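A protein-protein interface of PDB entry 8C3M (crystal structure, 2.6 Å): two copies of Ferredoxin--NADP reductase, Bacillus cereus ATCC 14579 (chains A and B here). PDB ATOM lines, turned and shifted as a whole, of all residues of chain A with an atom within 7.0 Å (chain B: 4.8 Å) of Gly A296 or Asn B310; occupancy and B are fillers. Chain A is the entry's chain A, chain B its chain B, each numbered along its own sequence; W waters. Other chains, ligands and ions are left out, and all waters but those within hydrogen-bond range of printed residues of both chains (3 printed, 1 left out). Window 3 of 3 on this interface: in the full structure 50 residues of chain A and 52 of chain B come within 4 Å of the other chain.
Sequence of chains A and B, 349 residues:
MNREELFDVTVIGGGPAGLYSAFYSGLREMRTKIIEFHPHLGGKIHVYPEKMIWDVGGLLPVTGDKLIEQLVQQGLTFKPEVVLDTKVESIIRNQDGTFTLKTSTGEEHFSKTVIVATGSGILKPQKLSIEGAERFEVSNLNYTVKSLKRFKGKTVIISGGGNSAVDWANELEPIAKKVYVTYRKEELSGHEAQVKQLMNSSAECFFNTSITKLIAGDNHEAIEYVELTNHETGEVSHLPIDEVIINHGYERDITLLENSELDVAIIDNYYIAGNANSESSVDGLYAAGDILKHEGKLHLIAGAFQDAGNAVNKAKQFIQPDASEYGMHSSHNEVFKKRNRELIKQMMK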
ATOM      1  N   ALA A 276      13.650  15.376  26.101  1.00  0.00           N
ATOM      2  CA  ALA A 276      13.883  16.047  27.372  1.00  0.00           C
ATOM      3  C   ALA A 276      13.978  15.070  28.513  1.00  0.00           C
ATOM      4  O   ALA A 276      14.288  15.494  29.625  1.00  0.00           O
ATOM      5  CB  ALA A 276      12.783  17.063  27.673  1.00  0.00           C
ATOM      6  N   LYS A 293      21.978  15.535  23.256  1.00  0.00           N
ATOM      7  CA  LYS A 293      21.594  16.778  22.607  1.00  0.00           C
ATOM      8  C   LYS A 293      20.082  16.811  22.465  1.00  0.00           C
ATOM      9  O   LYS A 293      19.497  15.848  21.989  1.00  0.00           O
ATOM     10  CB  LYS A 293      22.279  16.937  21.251  1.00  0.00           C
ATOM     11  CG  LYS A 293      22.493  18.374  20.910  1.00  0.00           C
ATOM     12  CD  LYS A 293      23.212  18.570  19.592  1.00  0.00           C
ATOM     13  CE  LYS A 293      22.991  19.992  19.016  1.00  0.00           C
ATOM     14  NZ  LYS A 293      23.896  20.290  17.846  1.00  0.00           N
ATOM     15  N   HIS A 294      19.453  17.862  22.971  1.00  0.00           N
ATOM     16  CA  HIS A 294      18.040  18.154  22.745  1.00  0.00           C
ATOM     17  C   HIS A 294      17.854  19.629  23.071  1.00  0.00           C
ATOM     18  O   HIS A 294      18.756  20.265  23.608  1.00  0.00           O
ATOM     19  CB  HIS A 294      17.108  17.256  23.567  1.00  0.00           C
ATOM     20  CG  HIS A 294      17.150  17.524  25.038  1.00  0.00           C
ATOM     21  ND1 HIS A 294      16.415  18.528  25.632  1.00  0.00           N
ATOM     22  CD2 HIS A 294      17.846  16.928  26.033  1.00  0.00           C
ATOM     23  CE1 HIS A 294      16.666  18.552  26.927  1.00  0.00           C
ATOM     24  NE2 HIS A 294      17.529  17.589  27.196  1.00  0.00           N
ATOM     25  N   GLU A 295      16.682  20.169  22.731  1.00  0.00           N
ATOM     26  CA  GLU A 295      16.468  21.616  22.750  1.00  0.00           C
ATOM     27  C   GLU A 295      16.669  22.233  24.129  1.00  0.00           C
ATOM     28  O   GLU A 295      16.944  23.437  24.214  1.00  0.00           O
ATOM     29  CB  GLU A 295      15.069  21.960  22.215  1.00  0.00           C
ATOM     30  CG  GLU A 295      14.789  23.474  22.010  1.00  0.00           C
ATOM     31  CD  GLU A 295      13.525  23.784  21.173  1.00  0.00           C
ATOM     32  OE1 GLU A 295      12.660  22.898  21.027  1.00  0.00           O
ATOM     33  OE2 GLU A 295      13.412  24.903  20.615  1.00  0.00           O
ATOM     34  N   GLY A 296      16.547  21.463  25.212  1.00  0.00           N
ATOM     35  CA  GLY A 296      16.741  22.020  26.542  1.00  0.00           C
ATOM     36  C   GLY A 296      17.982  21.551  27.273  1.00  0.00           C
ATOM     37  O   GLY A 296      18.078  21.750  28.491  1.00  0.00           O
ATOM     38  N   LYS A 297      18.916  20.899  26.592  1.00  0.00           N
ATOM     39  CA  LYS A 297      20.143  20.449  27.207  1.00  0.00           C
ATOM     40  C   LYS A 297      20.968  21.634  27.724  1.00  0.00           C
ATOM     41  O   LYS A 297      21.233  22.606  27.005  1.00  0.00           O
ATOM     42  CB  LYS A 297      20.902  19.617  26.185  1.00  0.00           C
ATOM     43  CG  LYS A 297      22.317  19.364  26.501  1.00  0.00           C
ATOM     44  CD  LYS A 297      22.444  18.551  27.714  1.00  0.00           C
ATOM     45  CE  LYS A 297      23.899  18.630  28.158  1.00  0.00           C
ATOM     46  NZ  LYS A 297      24.048  18.078  29.496  1.00  0.00           N
ATOM     47  N   LEU A 298      21.348  21.558  28.998  1.00  0.00           N
ATOM     48  CA  LEU A 298      22.120  22.591  29.656  1.00  0.00           C
ATOM     49  C   LEU A 298      23.568  22.119  29.680  1.00  0.00           C
ATOM     50  O   LEU A 298      23.856  21.032  30.186  1.00  0.00           O
ATOM     51  CB  LEU A 298      21.593  22.833  31.065  1.00  0.00           C
ATOM     52  CG  LEU A 298      22.378  23.874  31.858  1.00  0.00           C
ATOM     53  CD1 LEU A 298      22.324  25.292  31.183  1.00  0.00           C
ATOM     54  CD2 LEU A 298      21.852  23.914  33.297  1.00  0.00           C
ATOM     55  N   HIS A 299      24.457  22.898  29.074  1.00  0.00           N
ATOM     56  CA  HIS A 299      25.850  22.514  28.889  1.00  0.00           C
ATOM     57  C   HIS A 299      26.679  22.812  30.136  1.00  0.00           C
ATOM     58  O   HIS A 299      27.663  23.561  30.094  1.00  0.00           O
ATOM     59  CB  HIS A 299      26.420  23.230  27.667  1.00  0.00           C
ATOM     60  CG  HIS A 299      25.939  22.658  26.380  1.00  0.00           C
ATOM     61  ND1 HIS A 299      24.967  23.264  25.612  1.00  0.00           N
ATOM     62  CD2 HIS A 299      26.248  21.499  25.755  1.00  0.00           C
ATOM     63  CE1 HIS A 299      24.726  22.527  24.545  1.00  0.00           C
ATOM     64  NE2 HIS A 299      25.488  21.447  24.609  1.00  0.00           N
ATOM     65  N   GLN A 306      20.750  16.469  35.760  1.00  0.00           N
ATOM     66  CA  GLN A 306      19.366  16.334  35.313  1.00  0.00           C
ATOM     67  C   GLN A 306      19.243  15.252  34.258  1.00  0.00           C
ATOM     68  O   GLN A 306      18.342  14.416  34.343  1.00  0.00           O
ATOM     69  CB  GLN A 306      18.831  17.654  34.770  1.00  0.00           C
ATOM     70  CG  GLN A 306      17.582  17.467  33.912  1.00  0.00           C
ATOM     71  CD  GLN A 306      16.453  18.397  34.326  1.00  0.00           C
ATOM     72  OE1 GLN A 306      16.457  18.944  35.445  1.00  0.00           O
ATOM     73  NE2 GLN A 306      15.495  18.619  33.412  1.00  0.00           N
ATOM     74  N   ASP A 307      20.158  15.236  33.271  1.00  0.00           N
ATOM     75  CA  ASP A 307      20.137  14.182  32.254  1.00  0.00           C
ATOM     76  C   ASP A 307      20.195  12.829  32.916  1.00  0.00           C
ATOM     77  O   ASP A 307      19.416  11.926  32.577  1.00  0.00           O
ATOM     78  CB  ASP A 307      21.307  14.287  31.270  1.00  0.00           C
ATOM     79  CG  ASP A 307      21.394  15.637  30.568  1.00  0.00           C
ATOM     80  OD1 ASP A 307      20.357  16.361  30.449  1.00  0.00           O
ATOM     81  OD2 ASP A 307      22.533  15.984  30.148  1.00  0.00           O
ATOM     82  N   ALA B 276      11.047  22.783  27.780  1.00  0.00           N
ATOM     83  CA  ALA B 276      12.291  22.233  28.310  1.00  0.00           C
ATOM     84  C   ALA B 276      13.330  23.308  28.578  1.00  0.00           C
ATOM     85  O   ALA B 276      14.397  22.983  29.122  1.00  0.00           O
ATOM     86  CB  ALA B 276      12.879  21.206  27.348  1.00  0.00           C
ATOM     87  N   ASN B 277      13.049  24.554  28.185  1.00  0.00           N
ATOM     88  CA  ASN B 277      13.948  25.670  28.378  1.00  0.00           C
ATOM     89  C   ASN B 277      13.424  26.628  29.427  1.00  0.00           C
ATOM     90  O   ASN B 277      13.989  27.704  29.602  1.00  0.00           O
ATOM     91  CB  ASN B 277      14.189  26.375  27.043  1.00  0.00           C
ATOM     92  CG  ASN B 277      15.352  25.758  26.267  1.00  0.00           C
ATOM     93  OD1 ASN B 277      16.499  25.828  26.715  1.00  0.00           O
ATOM     94  ND2 ASN B 277      15.068  25.138  25.139  1.00  0.00           N
ATOM     95  N   SER B 278      12.395  26.219  30.173  1.00  0.00           N
ATOM     96  CA  SER B 278      11.814  26.966  31.287  1.00  0.00           C
ATOM     97  C   SER B 278      10.979  28.157  30.834  1.00  0.00           C
ATOM     98  O   SER B 278      10.652  29.032  31.653  1.00  0.00           O
ATOM     99  CB  SER B 278      12.895  27.438  32.269  1.00  0.00           C
ATOM    100  OG  SER B 278      13.771  26.377  32.635  1.00  0.00           O
ATOM    101  N   GLN B 306      18.808  22.993  36.961  1.00  0.00           N
ATOM    102  CA  GLN B 306      18.707  22.972  35.510  1.00  0.00           C
ATOM    103  C   GLN B 306      17.647  23.954  35.016  1.00  0.00           C
ATOM    104  O   GLN B 306      17.885  24.664  34.037  1.00  0.00           O
ATOM    105  CB  GLN B 306      18.426  21.563  35.002  1.00  0.00           C
ATOM    106  CG  GLN B 306      17.835  21.600  33.592  1.00  0.00           C
ATOM    107  CD  GLN B 306      18.586  20.753  32.607  1.00  0.00           C
ATOM    108  OE1 GLN B 306      19.733  20.383  32.841  1.00  0.00           O
ATOM    109  NE2 GLN B 306      17.943  20.440  31.480  1.00  0.00           N
ATOM    110  N   ASP B 307      16.468  23.993  35.660  1.00  0.00           N
ATOM    111  CA  ASP B 307      15.435  24.971  35.298  1.00  0.00           C
ATOM    112  C   ASP B 307      15.984  26.389  35.381  1.00  0.00           C
ATOM    113  O   ASP B 307      15.822  27.194  34.455  1.00  0.00           O
ATOM    114  CB  ASP B 307      14.221  24.864  36.224  1.00  0.00           C
ATOM    115  CG  ASP B 307      13.634  23.456  36.289  1.00  0.00           C
ATOM    116  OD1 ASP B 307      13.869  22.664  35.336  1.00  0.00           O
ATOM    117  OD2 ASP B 307      12.931  23.152  37.291  1.00  0.00           O
ATOM    118  N   ALA B 308      16.645  26.702  36.499  1.00  0.00           N
ATOM    119  CA  ALA B 308      17.159  28.038  36.726  1.00  0.00           C
ATOM    120  C   ALA B 308      18.169  28.418  35.651  1.00  0.00           C
ATOM    121  O   ALA B 308      18.054  29.476  35.035  1.00  0.00           O
ATOM    122  CB  ALA B 308      17.771  28.108  38.127  1.00  0.00           C
ATOM    123  N   GLY B 309      19.171  27.570  35.415  1.00  0.00           N
ATOM    124  CA  GLY B 309      20.133  27.855  34.361  1.00  0.00           C
ATOM    125  C   GLY B 309      19.474  28.035  32.998  1.00  0.00           C
ATOM    126  O   GLY B 309      19.810  28.968  32.247  1.00  0.00           O
ATOM    127  N   ASN B 310      18.531  27.141  32.646  1.00  0.00           N
ATOM    128  CA  ASN B 310      17.847  27.312  31.368  1.00  0.00           C
ATOM    129  C   ASN B 310      17.050  28.623  31.326  1.00  0.00           C
ATOM    130  O   ASN B 310      17.068  29.340  30.323  1.00  0.00           O
ATOM    131  CB  ASN B 310      16.933  26.122  31.081  1.00  0.00           C
ATOM    132  CG  ASN B 310      17.650  25.015  30.336  1.00  0.00           C
ATOM    133  OD1 ASN B 310      18.742  25.235  29.801  1.00  0.00           O
ATOM    134  ND2 ASN B 310      17.043  23.837  30.276  1.00  0.00           N
ATOM    135  N   ALA B 311      16.353  28.954  32.410  1.00  0.00           N
ATOM    136  CA  ALA B 311      15.609  30.197  32.465  1.00  0.00           C
ATOM    137  C   ALA B 311      16.532  31.395  32.284  1.00  0.00           C
ATOM    138  O   ALA B 311      16.267  32.288  31.462  1.00  0.00           O
ATOM    139  CB  ALA B 311      14.862  30.276  33.791  1.00  0.00           C
ATOM    140  N   VAL B 312      17.630  31.431  33.049  1.00  0.00           N
ATOM    141  CA  VAL B 312      18.528  32.581  33.012  1.00  0.00           C
ATOM    142  C   VAL B 312      19.125  32.734  31.620  1.00  0.00           C
ATOM    143  O   VAL B 312      19.260  33.854  31.110  1.00  0.00           O
ATOM    144  CB  VAL B 312      19.620  32.457  34.106  1.00  0.00           C
ATOM    145  CG1 VAL B 312      20.791  33.444  33.862  1.00  0.00           C
ATOM    146  CG2 VAL B 312      19.026  32.633  35.510  1.00  0.00           C
ATOM    147  N   ASN B 313      19.524  31.622  30.995  1.00  0.00           N
ATOM    148  CA  ASN B 313      20.123  31.712  29.666  1.00  0.00           C
ATOM    149  C   ASN B 313      19.134  32.260  28.651  1.00  0.00           C
ATOM    150  O   ASN B 313      19.503  33.031  27.755  1.00  0.00           O
ATOM    151  CB  ASN B 313      20.672  30.356  29.235  1.00  0.00           C
ATOM    152  CG  ASN B 313      22.124  30.157  29.651  1.00  0.00           C
ATOM    153  OD1 ASN B 313      22.889  31.115  29.726  1.00  0.00           O
ATOM    154  ND2 ASN B 313      22.525  28.916  29.855  1.00  0.00           N
ATOM    155  N   LYS B 314      17.862  31.917  28.796  1.00  0.00           N
ATOM    156  CA  LYS B 314      16.874  32.489  27.893  1.00  0.00           C
ATOM    157  C   LYS B 314      16.670  33.960  28.182  1.00  0.00           C
ATOM    158  O   LYS B 314      16.585  34.768  27.251  1.00  0.00           O
ATOM    159  CB  LYS B 314      15.552  31.743  28.011  1.00  0.00           C
ATOM    160  CG  LYS B 314      15.545  30.431  27.310  1.00  0.00           C
ATOM    161  CD  LYS B 314      15.992  30.590  25.875  1.00  0.00           C
ATOM    162  CE  LYS B 314      15.667  29.332  25.069  1.00  0.00           C
ATOM    163  NZ  LYS B 314      15.968  29.515  23.620  1.00  0.00           N
HETATM  164  O   HOH W   1      13.807  20.103  36.011  1.00  0.00           O
HETATM  165  O   HOH W   2      20.928  19.436  30.561  1.00  0.00           O
HETATM  166  O   HOH W   3      14.030  21.647  32.963  1.00  0.00           O
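NE2 of Gln B306 is in hydrogen-bond range of O of Gly A296 (3.3 Å).
The backbone carbonyl oxygen (O) of Gly A296 is in hydrogen-bond range of the side-chain amide nitrogen (ND2) of Asn B310, at 2.9 Å.
The backbone carbonyl oxygen (O) of Glu A295 is in hydrogen-bond range of the side-chain amide nitrogen (ND2) of Asn B277, at 2.7 Å.
Gln A306 touches its own counterpart, Gln B306.
Of the 9 pairs that touch across the chains among the printed residues, 1 has its exchanged pair printed and touching as well.
Printed residues of chain A that touch a printed residue of chain B: Glu A295, Gly A296, Leu A298 and Gln A306.
Printed residues of chain B that touch a printed residue of chain A: Ala B276, Asn B277, Gln B306, Asn B310 and Asn B313.
Along chain B the printed residues that touch a printed residue of chain A span positions 276 to 313.
Among the printed residues, no Asp or Glu carboxylate lies within 4 Å of a Lys or Arg side-chain nitrogen of the other chain.
Water W3 bridges the side-chain carboxylate (OD1) of Asp B307 and the side-chain amide nitrogen (NE2) of Gln A306.
Water W1 bridges the side-chain carboxylate of Asp B307 and the side-chain amide oxygen of Gln A306.
Water W2 lies within hydrogen-bond range of the backbone NH (N) of Leu A298 (2.7 Å), the side-chain amide oxygen (OE1) of Gln B306 (2.7 Å) and the side-chain carboxylate (OD1) of Asp A307 (3.1 Å).
O of Ala B276 lies within hydrogen-bond range of ND2 of Asn B310 (3.0 Å).
N of Gly A296 is in hydrogen-bond range of ND1 of His A294 (3.0 Å).
His A294 touches none of the printed residues of chain B.
Gly A296 touches just these residues of chain B: Ala B276, Asn B277, Gln B306 and Asn B310.
Lys A297 touches none of the printed residues of chain B.
Of the printed residues of chain B, Leu A298 touches Gln B306, Asn B310 and Asn B313.
Of the printed residues of chain B, Gln A306 touches Gln B306.
Of the printed residues of chain A, Ala B276 touches Gly A296.
Of the printed residues of chain A, Gln B306 touches Gly A296 (3.3 Å), Leu A298 (3.6 Å) and Gln A306 (3.3 Å).
Of chain A, only Gly A296 (2.9 Å) and Leu A298 (3.8 Å) come within 4 Å of Asn B310.
Printed residues of chain A within 4 Å of Asn B313: Leu A298.
The nearest residue of chain A that does not touch Asn B310 is Lys A297 (4.6 Å).
The nearest printed residue of chain B that does not touch Leu A298 is Gly B309 (4.4 Å).
Among the printed residues, merely in contact across the chains: Gly A296 with Ala B276, Gly A296 with Asn B277, Leu A298 with Gln B306, Leu A298 with Asn B310, Leu A298 with Asn B313 and Gln A306 with Gln B306.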
